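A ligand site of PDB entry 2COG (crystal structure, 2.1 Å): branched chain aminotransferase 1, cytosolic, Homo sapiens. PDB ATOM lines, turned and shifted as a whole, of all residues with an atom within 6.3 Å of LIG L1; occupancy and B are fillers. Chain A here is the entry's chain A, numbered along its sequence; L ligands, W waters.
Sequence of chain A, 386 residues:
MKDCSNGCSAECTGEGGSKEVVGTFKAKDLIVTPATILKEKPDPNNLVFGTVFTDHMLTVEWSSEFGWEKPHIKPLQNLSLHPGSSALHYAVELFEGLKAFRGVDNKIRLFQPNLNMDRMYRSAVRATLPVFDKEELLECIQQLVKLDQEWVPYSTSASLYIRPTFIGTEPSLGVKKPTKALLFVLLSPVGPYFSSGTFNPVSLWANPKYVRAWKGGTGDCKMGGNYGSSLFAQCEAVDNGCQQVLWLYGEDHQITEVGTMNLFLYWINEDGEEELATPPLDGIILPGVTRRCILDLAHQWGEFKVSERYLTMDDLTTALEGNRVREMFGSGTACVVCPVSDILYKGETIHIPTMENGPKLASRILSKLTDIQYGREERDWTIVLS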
ATOM      1  N   PHE A  95     -30.504 -24.068  -8.627  1.00  0.00           N
ATOM      2  CA  PHE A  95     -30.065 -25.422  -8.904  1.00  0.00           C
ATOM      3  C   PHE A  95     -28.614 -25.627  -8.561  1.00  0.00           C
ATOM      4  O   PHE A  95     -27.932 -24.712  -8.104  1.00  0.00           O
ATOM      5  CB  PHE A  95     -30.303 -25.756 -10.384  1.00  0.00           C
ATOM      6  CG  PHE A  95     -29.476 -24.937 -11.338  1.00  0.00           C
ATOM      7  CD1 PHE A  95     -28.312 -25.455 -11.892  1.00  0.00           C
ATOM      8  CD2 PHE A  95     -29.866 -23.645 -11.693  1.00  0.00           C
ATOM      9  CE1 PHE A  95     -27.552 -24.696 -12.788  1.00  0.00           C
ATOM     10  CE2 PHE A  95     -29.112 -22.888 -12.576  1.00  0.00           C
ATOM     11  CZ  PHE A  95     -27.956 -23.410 -13.135  1.00  0.00           C
ATOM     12  N   GLU A  96     -28.153 -26.851  -8.772  1.00  0.00           N
ATOM     13  CA  GLU A  96     -26.772 -27.219  -8.534  1.00  0.00           C
ATOM     14  C   GLU A  96     -26.377 -28.235  -9.592  1.00  0.00           C
ATOM     15  O   GLU A  96     -27.227 -28.707 -10.365  1.00  0.00           O
ATOM     16  CB  GLU A  96     -26.617 -27.836  -7.141  1.00  0.00           C
ATOM     17  CG  GLU A  96     -26.178 -26.849  -6.075  1.00  0.00           C
ATOM     18  CD  GLU A  96     -24.909 -26.126  -6.467  1.00  0.00           C
ATOM     19  OE1 GLU A  96     -24.068 -26.730  -7.175  1.00  0.00           O
ATOM     20  OE2 GLU A  96     -24.743 -24.952  -6.069  1.00  0.00           O
ATOM     21  N   GLY A  97     -25.099 -28.581  -9.627  1.00  0.00           N
ATOM     22  CA  GLY A  97     -24.641 -29.541 -10.603  1.00  0.00           C
ATOM     23  C   GLY A  97     -23.329 -30.171 -10.191  1.00  0.00           C
ATOM     24  O   GLY A  97     -22.291 -29.494 -10.174  1.00  0.00           O
ATOM     25  N   ASN A 116     -20.902 -28.111  -3.076  1.00  0.00           N
ATOM     26  CA  ASN A 116     -22.159 -27.880  -3.771  1.00  0.00           C
ATOM     27  C   ASN A 116     -23.274 -27.654  -2.765  1.00  0.00           C
ATOM     28  O   ASN A 116     -24.155 -26.818  -2.989  1.00  0.00           O
ATOM     29  CB  ASN A 116     -22.499 -29.074  -4.653  1.00  0.00           C
ATOM     30  CG  ASN A 116     -21.618 -29.163  -5.876  1.00  0.00           C
ATOM     31  OD1 ASN A 116     -21.825 -28.453  -6.853  1.00  0.00           O
ATOM     32  ND2 ASN A 116     -20.616 -30.030  -5.811  1.00  0.00           N
ATOM     33  N   ARG A 119     -22.896 -24.046  -1.422  1.00  0.00           N
ATOM     34  CA  ARG A 119     -23.372 -23.100  -2.407  1.00  0.00           C
ATOM     35  C   ARG A 119     -24.903 -23.132  -2.495  1.00  0.00           C
ATOM     36  O   ARG A 119     -25.554 -22.083  -2.496  1.00  0.00           O
ATOM     37  CB  ARG A 119     -22.753 -23.405  -3.773  1.00  0.00           C
ATOM     38  CG  ARG A 119     -22.995 -22.328  -4.816  1.00  0.00           C
ATOM     39  CD  ARG A 119     -22.088 -22.541  -6.019  1.00  0.00           C
ATOM     40  NE  ARG A 119     -22.438 -23.725  -6.807  1.00  0.00           N
ATOM     41  CZ  ARG A 119     -21.630 -24.280  -7.694  1.00  0.00           C
ATOM     42  NH1 ARG A 119     -20.427 -23.762  -7.905  1.00  0.00           N
ATOM     43  NH2 ARG A 119     -22.019 -25.358  -8.378  1.00  0.00           N
ATOM     44  N   ARG A 212     -24.434 -10.116 -18.194  1.00  0.00           N
ATOM     45  CA  ARG A 212     -24.831 -11.276 -17.393  1.00  0.00           C
ATOM     46  C   ARG A 212     -25.189 -10.932 -15.944  1.00  0.00           C
ATOM     47  O   ARG A 212     -26.288 -11.208 -15.497  1.00  0.00           O
ATOM     48  CB  ARG A 212     -23.704 -12.323 -17.403  1.00  0.00           C
ATOM     49  CG  ARG A 212     -24.127 -13.714 -16.960  1.00  0.00           C
ATOM     50  CD  ARG A 212     -22.921 -14.643 -16.777  1.00  0.00           C
ATOM     51  NE  ARG A 212     -22.333 -14.514 -15.453  1.00  0.00           N
ATOM     52  CZ  ARG A 212     -22.893 -14.949 -14.319  1.00  0.00           C
ATOM     53  NH1 ARG A 212     -24.073 -15.556 -14.352  1.00  0.00           N
ATOM     54  NH2 ARG A 212     -22.266 -14.783 -13.158  1.00  0.00           N
ATOM     55  N   GLY A 219     -25.567 -12.670  -9.548  1.00  0.00           N
ATOM     56  CA  GLY A 219     -24.647 -13.414 -10.375  1.00  0.00           C
ATOM     57  C   GLY A 219     -23.741 -14.396  -9.657  1.00  0.00           C
ATOM     58  O   GLY A 219     -23.188 -15.303 -10.280  1.00  0.00           O
ATOM     59  N   CYS A 221     -24.712 -16.449  -7.365  1.00  0.00           N
ATOM     60  CA  CYS A 221     -25.542 -17.527  -6.870  1.00  0.00           C
ATOM     61  C   CYS A 221     -26.040 -18.295  -8.092  1.00  0.00           C
ATOM     62  O   CYS A 221     -26.098 -17.736  -9.191  1.00  0.00           O
ATOM     63  CB  CYS A 221     -26.740 -16.998  -6.073  1.00  0.00           C
ATOM     64  SG  CYS A 221     -26.311 -16.125  -4.568  1.00  0.00           S
ATOM     65  N   LYS A 222     -26.387 -19.555  -7.892  1.00  0.00           N
ATOM     66  CA  LYS A 222     -26.879 -20.371  -8.995  1.00  0.00           C
ATOM     67  C   LYS A 222     -28.408 -20.330  -9.041  1.00  0.00           C
ATOM     68  O   LYS A 222     -29.083 -21.345  -8.929  1.00  0.00           O
ATOM     69  CB  LYS A 222     -26.367 -21.804  -8.876  1.00  0.00           C
ATOM     70  CG  LYS A 222     -25.494 -22.242 -10.039  1.00  0.00           C
ATOM     71  CD  LYS A 222     -24.890 -23.637  -9.828  1.00  0.00           C
ATOM     72  CE  LYS A 222     -24.401 -24.233 -11.151  1.00  0.00           C
ATOM     73  NZ  LYS A 222     -23.539 -23.224 -11.769  1.00  0.00           N
ATOM     74  N   TYR A 227     -30.061 -17.126 -15.744  1.00  0.00           N
ATOM     75  CA  TYR A 227     -29.807 -17.895 -16.948  1.00  0.00           C
ATOM     76  C   TYR A 227     -30.806 -17.722 -18.074  1.00  0.00           C
ATOM     77  O   TYR A 227     -30.430 -17.748 -19.249  1.00  0.00           O
ATOM     78  CB  TYR A 227     -29.689 -19.385 -16.584  1.00  0.00           C
ATOM     79  CG  TYR A 227     -28.624 -19.618 -15.539  1.00  0.00           C
ATOM     80  CD1 TYR A 227     -28.851 -19.253 -14.202  1.00  0.00           C
ATOM     81  CD2 TYR A 227     -27.354 -20.092 -15.882  1.00  0.00           C
ATOM     82  CE1 TYR A 227     -27.849 -19.358 -13.249  1.00  0.00           C
ATOM     83  CE2 TYR A 227     -26.336 -20.188 -14.920  1.00  0.00           C
ATOM     84  CZ  TYR A 227     -26.588 -19.812 -13.615  1.00  0.00           C
ATOM     85  OH  TYR A 227     -25.591 -19.839 -12.677  1.00  0.00           O
ATOM     86  N   GLU A 257     -16.898 -14.261 -17.467  1.00  0.00           N
ATOM     87  CA  GLU A 257     -17.131 -15.688 -17.616  1.00  0.00           C
ATOM     88  C   GLU A 257     -17.354 -16.135 -19.046  1.00  0.00           C
ATOM     89  O   GLU A 257     -17.694 -15.336 -19.918  1.00  0.00           O
ATOM     90  CB  GLU A 257     -18.319 -16.096 -16.732  1.00  0.00           C
ATOM     91  CG  GLU A 257     -18.013 -15.997 -15.249  1.00  0.00           C
ATOM     92  CD  GLU A 257     -19.012 -16.745 -14.388  1.00  0.00           C
ATOM     93  OE1 GLU A 257     -19.396 -17.865 -14.785  1.00  0.00           O
ATOM     94  OE2 GLU A 257     -19.378 -16.233 -13.309  1.00  0.00           O
ATOM     95  N   GLY A 259     -19.696 -18.189 -21.057  1.00  0.00           N
ATOM     96  CA  GLY A 259     -20.974 -18.879 -21.045  1.00  0.00           C
ATOM     97  C   GLY A 259     -21.297 -19.203 -19.590  1.00  0.00           C
ATOM     98  O   GLY A 259     -21.355 -18.312 -18.760  1.00  0.00           O
ATOM     99  N   THR A 260     -21.483 -20.493 -19.292  1.00  0.00           N
ATOM    100  CA  THR A 260     -21.786 -20.925 -17.928  1.00  0.00           C
ATOM    101  C   THR A 260     -20.525 -21.442 -17.208  1.00  0.00           C
ATOM    102  O   THR A 260     -20.624 -22.256 -16.309  1.00  0.00           O
ATOM    103  CB  THR A 260     -22.849 -22.062 -17.913  1.00  0.00           C
ATOM    104  OG1 THR A 260     -22.325 -23.231 -18.560  1.00  0.00           O
ATOM    105  CG2 THR A 260     -24.112 -21.617 -18.612  1.00  0.00           C
ATOM    106  N   MET A 261     -19.354 -20.962 -17.610  1.00  0.00           N
ATOM    107  CA  MET A 261     -18.103 -21.419 -17.008  1.00  0.00           C
ATOM    108  C   MET A 261     -17.181 -20.274 -16.597  1.00  0.00           C
ATOM    109  O   MET A 261     -17.219 -19.193 -17.195  1.00  0.00           O
ATOM    110  CB  MET A 261     -17.321 -22.289 -17.987  1.00  0.00           C
ATOM    111  CG  MET A 261     -18.007 -23.574 -18.396  1.00  0.00           C
ATOM    112  SD  MET A 261     -17.037 -24.358 -19.682  1.00  0.00           S
ATOM    113  CE  MET A 261     -17.720 -23.546 -21.147  1.00  0.00           C
ATOM    114  N   ASN A 262     -16.358 -20.537 -15.591  1.00  0.00           N
ATOM    115  CA  ASN A 262     -15.407 -19.529 -15.131  1.00  0.00           C
ATOM    116  C   ASN A 262     -14.280 -19.486 -16.135  1.00  0.00           C
ATOM    117  O   ASN A 262     -13.944 -20.499 -16.748  1.00  0.00           O
ATOM    118  CB  ASN A 262     -14.891 -19.878 -13.744  1.00  0.00           C
ATOM    119  CG  ASN A 262     -15.962 -19.733 -12.698  1.00  0.00           C
ATOM    120  OD1 ASN A 262     -16.445 -18.632 -12.449  1.00  0.00           O
ATOM    121  ND2 ASN A 262     -16.352 -20.846 -12.081  1.00  0.00           N
ATOM    122  N   LEU A 286     -19.639 -16.312 -10.558  1.00  0.00           N
ATOM    123  CA  LEU A 286     -20.134 -17.427  -9.758  1.00  0.00           C
ATOM    124  C   LEU A 286     -18.949 -18.275  -9.309  1.00  0.00           C
ATOM    125  O   LEU A 286     -18.149 -18.731 -10.119  1.00  0.00           O
ATOM    126  CB  LEU A 286     -21.113 -18.284 -10.561  1.00  0.00           C
ATOM    127  CG  LEU A 286     -21.783 -19.316  -9.645  1.00  0.00           C
ATOM    128  CD1 LEU A 286     -23.271 -19.363  -9.901  1.00  0.00           C
ATOM    129  CD2 LEU A 286     -21.129 -20.671  -9.856  1.00  0.00           C
ATOM    130  N   PRO A 287     -18.820 -18.481  -7.992  1.00  0.00           N
ATOM    131  CA  PRO A 287     -17.708 -19.280  -7.460  1.00  0.00           C
ATOM    132  C   PRO A 287     -17.852 -20.763  -7.799  1.00  0.00           C
ATOM    133  O   PRO A 287     -18.488 -21.519  -7.053  1.00  0.00           O
ATOM    134  CB  PRO A 287     -17.762 -18.995  -5.960  1.00  0.00           C
ATOM    135  CG  PRO A 287     -19.233 -18.752  -5.720  1.00  0.00           C
ATOM    136  CD  PRO A 287     -19.646 -17.922  -6.905  1.00  0.00           C
ATOM    137  N   GLY A 288     -17.250 -21.159  -8.908  1.00  0.00           N
ATOM    138  CA  GLY A 288     -17.337 -22.538  -9.345  1.00  0.00           C
ATOM    139  C   GLY A 288     -16.484 -23.500  -8.534  1.00  0.00           C
ATOM    140  O   GLY A 288     -15.452 -23.121  -7.988  1.00  0.00           O
ATOM    141  N   VAL A 289     -16.937 -24.742  -8.450  1.00  0.00           N
ATOM    142  CA  VAL A 289     -16.218 -25.773  -7.718  1.00  0.00           C
ATOM    143  C   VAL A 289     -14.938 -26.148  -8.487  1.00  0.00           C
ATOM    144  O   VAL A 289     -13.934 -26.510  -7.894  1.00  0.00           O
ATOM    145  CB  VAL A 289     -17.076 -27.036  -7.554  1.00  0.00           C
ATOM    146  CG1 VAL A 289     -16.256 -28.148  -6.900  1.00  0.00           C
ATOM    147  CG2 VAL A 289     -18.309 -26.717  -6.730  1.00  0.00           C
ATOM    148  N   THR A 290     -14.995 -26.047  -9.813  1.00  0.00           N
ATOM    149  CA  THR A 290     -13.832 -26.363 -10.629  1.00  0.00           C
ATOM    150  C   THR A 290     -12.822 -25.239 -10.543  1.00  0.00           C
ATOM    151  O   THR A 290     -11.610 -25.460 -10.577  1.00  0.00           O
ATOM    152  CB  THR A 290     -14.220 -26.593 -12.095  1.00  0.00           C
ATOM    153  OG1 THR A 290     -15.340 -27.486 -12.173  1.00  0.00           O
ATOM    154  CG2 THR A 290     -13.058 -27.212 -12.860  1.00  0.00           C
ATOM    155  N   ARG A 291     -13.337 -24.018 -10.430  1.00  0.00           N
ATOM    156  CA  ARG A 291     -12.522 -22.829 -10.329  1.00  0.00           C
ATOM    157  C   ARG A 291     -11.679 -22.926  -9.048  1.00  0.00           C
ATOM    158  O   ARG A 291     -10.477 -22.651  -9.065  1.00  0.00           O
ATOM    159  CB  ARG A 291     -13.410 -21.587 -10.247  1.00  0.00           C
ATOM    160  CG  ARG A 291     -12.704 -20.282  -9.911  1.00  0.00           C
ATOM    161  CD  ARG A 291     -13.697 -19.134  -9.893  1.00  0.00           C
ATOM    162  NE  ARG A 291     -13.088 -17.831  -9.650  1.00  0.00           N
ATOM    163  CZ  ARG A 291     -12.654 -17.414  -8.466  1.00  0.00           C
ATOM    164  NH1 ARG A 291     -12.767 -18.197  -7.399  1.00  0.00           N
ATOM    165  NH2 ARG A 291     -12.105 -16.205  -8.339  1.00  0.00           N
ATOM    166  N   SER A 331     -13.910 -23.305 -17.228  1.00  0.00           N
ATOM    167  CA  SER A 331     -13.934 -24.423 -16.300  1.00  0.00           C
ATOM    168  C   SER A 331     -15.341 -24.582 -15.734  1.00  0.00           C
ATOM    169  O   SER A 331     -16.032 -23.582 -15.518  1.00  0.00           O
ATOM    170  CB  SER A 331     -12.954 -24.184 -15.135  1.00  0.00           C
ATOM    171  OG  SER A 331     -13.456 -23.198 -14.237  1.00  0.00           O
ATOM    172  N   GLY A 332     -15.745 -25.817 -15.481  1.00  0.00           N
ATOM    173  CA  GLY A 332     -17.061 -26.088 -14.949  1.00  0.00           C
ATOM    174  C   GLY A 332     -17.295 -27.583 -14.780  1.00  0.00           C
ATOM    175  O   GLY A 332     -16.530 -28.398 -15.282  1.00  0.00           O
ATOM    176  N   THR A 333     -18.345 -27.957 -14.072  1.00  0.00           N
ATOM    177  CA  THR A 333     -18.612 -29.367 -13.857  1.00  0.00           C
ATOM    178  C   THR A 333     -18.833 -30.150 -15.147  1.00  0.00           C
ATOM    179  O   THR A 333     -18.365 -31.284 -15.276  1.00  0.00           O
ATOM    180  CB  THR A 333     -19.813 -29.568 -12.935  1.00  0.00           C
ATOM    181  OG1 THR A 333     -19.510 -29.061 -11.629  1.00  0.00           O
ATOM    182  CG2 THR A 333     -20.176 -31.058 -12.832  1.00  0.00           C
ATOM    183  N   ALA A 334     -19.526 -29.534 -16.100  1.00  0.00           N
ATOM    184  CA  ALA A 334     -19.826 -30.174 -17.382  1.00  0.00           C
ATOM    185  C   ALA A 334     -18.626 -30.334 -18.309  1.00  0.00           C
ATOM    186  O   ALA A 334     -18.483 -31.366 -18.968  1.00  0.00           O
ATOM    187  CB  ALA A 334     -20.924 -29.397 -18.089  1.00  0.00           C
HETATM  188  N1  LIG L   1     -20.397 -20.034 -13.934  1.00  0.00           N
HETATM  189  C1  LIG L   1     -21.758 -20.082 -13.908  1.00  0.00           C
HETATM  190  C2  LIG L   1     -22.570 -18.840 -14.366  1.00  0.00           C
HETATM  191  C3  LIG L   1     -22.383 -21.219 -13.453  1.00  0.00           C
HETATM  192  O1  LIG L   1     -23.752 -21.295 -13.431  1.00  0.00           O
HETATM  193  C4  LIG L   1     -21.640 -22.305 -13.036  1.00  0.00           C
HETATM  194  C5  LIG L   1     -22.418 -23.531 -12.522  1.00  0.00           C
HETATM  195  C6  LIG L   1     -20.231 -22.223 -13.086  1.00  0.00           C
HETATM  196  C7  LIG L   1     -19.648 -21.084 -13.536  1.00  0.00           C
HETATM  197  C8  LIG L   1     -19.287 -23.372 -12.696  1.00  0.00           C
HETATM  198  O2  LIG L   1     -19.278 -23.864 -11.379  1.00  0.00           O
HETATM  199  P1  LIG L   1     -18.781 -25.386 -11.178  1.00  0.00           P
HETATM  200  O3  LIG L   1     -19.594 -26.325 -11.996  1.00  0.00           O
HETATM  201  O4  LIG L   1     -19.212 -25.464  -9.647  1.00  0.00           O
HETATM  202  O5  LIG L   1     -17.300 -25.402 -11.308  1.00  0.00           O
HETATM  203  C1  LG2 L   2     -22.746 -25.795 -15.658  1.00  0.00           C
HETATM  204  C2  LG2 L   2     -23.835 -26.285 -16.634  1.00  0.00           C
HETATM  205  C3  LG2 L   2     -25.274 -25.884 -16.243  1.00  0.00           C
HETATM  206  C4  LG2 L   2     -25.382 -24.363 -16.178  1.00  0.00           C
HETATM  207  C5  LG2 L   2     -26.257 -26.438 -17.258  1.00  0.00           C
HETATM  208  C6  LG2 L   2     -21.345 -26.208 -16.061  1.00  0.00           C
HETATM  209  O1  LG2 L   2     -20.910 -27.310 -15.645  1.00  0.00           O
HETATM  210  O2  LG2 L   2     -20.670 -25.431 -16.784  1.00  0.00           O
HETATM  211  O   HOH W   1     -22.128 -26.930 -11.262  1.00  0.00           O
HETATM  212  O   HOH W   2     -19.888 -28.115  -8.992  1.00  0.00           O
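A carbon (C5) of LIG L1 is covalently linked to the side-chain amino group (NZ) of Lys 222, 1.4 Å away.
The side-chain hydroxyl (OH) of Tyr 227 lies close to an oxygen (O1) of LIG L1, 2.5 Å away.
The side-chain carboxylate (OE1) of Glu 257 lies close to a nitrogen (N1) of LIG L1, at 2.5 Å.
O4 of LIG L1 lies close to N of Val 289, at 2.7 Å.
NH1 of Arg 119 lies close to O4 of LIG L1 (2.7 Å).
N of Thr 333 sits close to O3 of LIG L1, 2.9 Å away.
An oxygen (O3) of LIG L1 lies close to the side-chain hydroxyl (OG1) of Thr 333 (2.8 Å).
O5 of LIG L1 sits close to N of Thr 290, 2.8 Å away.
The side-chain hydroxyl (OG1) of Thr 290 sits close to an oxygen (O5) of LIG L1 (3.0 Å).
O of Thr 260 lies close to N1 of LIG L1, at 3.3 Å.
N of Thr 333 sits close to O1 of LG2 L2 (3.1 Å).
The backbone carbonyl oxygen (O) of Thr 260 lies close to an oxygen (O2) of LG2 L2, at 3.2 Å.
An oxygen (O2) of LG2 L2 lies close to the side-chain hydroxyl (OG1) of Thr 260, 3.3 Å away.
O1 of LG2 L2 sits close to N of Ala 334.
OE2 of Glu 257 lies within salt-bridge range of NH2 of Arg 212 (3.2 Å).
The backbone NH of Leu 286 sits at hydrogen-bond distance from the side-chain carboxylate of Glu 257, 2.8 Å away.
The guanidinium group of Arg 119 lies within hydrogen-bond range of the backbone carbonyl oxygen of Pro 287, at 3.1 Å.
NH2 of Arg 119 lies within hydrogen-bond range of OD1 of Asn 116.
The guanidinium group (NE) of Arg 119 lies within salt-bridge range of the side-chain carboxylate (OE2) of Glu 96, at 2.7 Å.
The backbone carbonyl oxygen (O) of Gly 97 lies within hydrogen-bond range of the side-chain hydroxyl (OG1) of Thr 333, at 3.2 Å.
N of Gly 288 sits close to ND2 of Asn 262.
The backbone NH of Ser 331 is in hydrogen-bond range of the backbone carbonyl oxygen of Asn 262 (2.8 Å).
NH1 of Arg 212 touches C2 of LIG L1, 3.6 Å away.
CA of Met 261 touches C7 of LIG L1, 3.8 Å away.
ND2 of Asn 262 touches C7 of LIG L1 (3.6 Å).
CD2 of Leu 286 touches C4 of LIG L1 (3.6 Å).
CA of Gly 288 touches O2 of LIG L1, at 3.1 Å.
Gly 332 touches LIG L1 (CA to O5, 3.7 Å).
The nearest printed residue that does not touch LIG L1 is Arg 291 (4.3 Å).
Water W1 lies within hydrogen-bond range of the backbone carbonyl oxygen (O) of Gly 97 (2.8 Å), the guanidinium group (NH2) of Arg 119 (3.3 Å) and the side-chain hydroxyl (OG1) of Thr 333 (3.4 Å).
Water W2 lies within hydrogen-bond range of OG1 of Thr 333 (2.8 Å), OD1 of Asn 116 (2.9 Å) and O of Gly 97 (3.0 Å).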
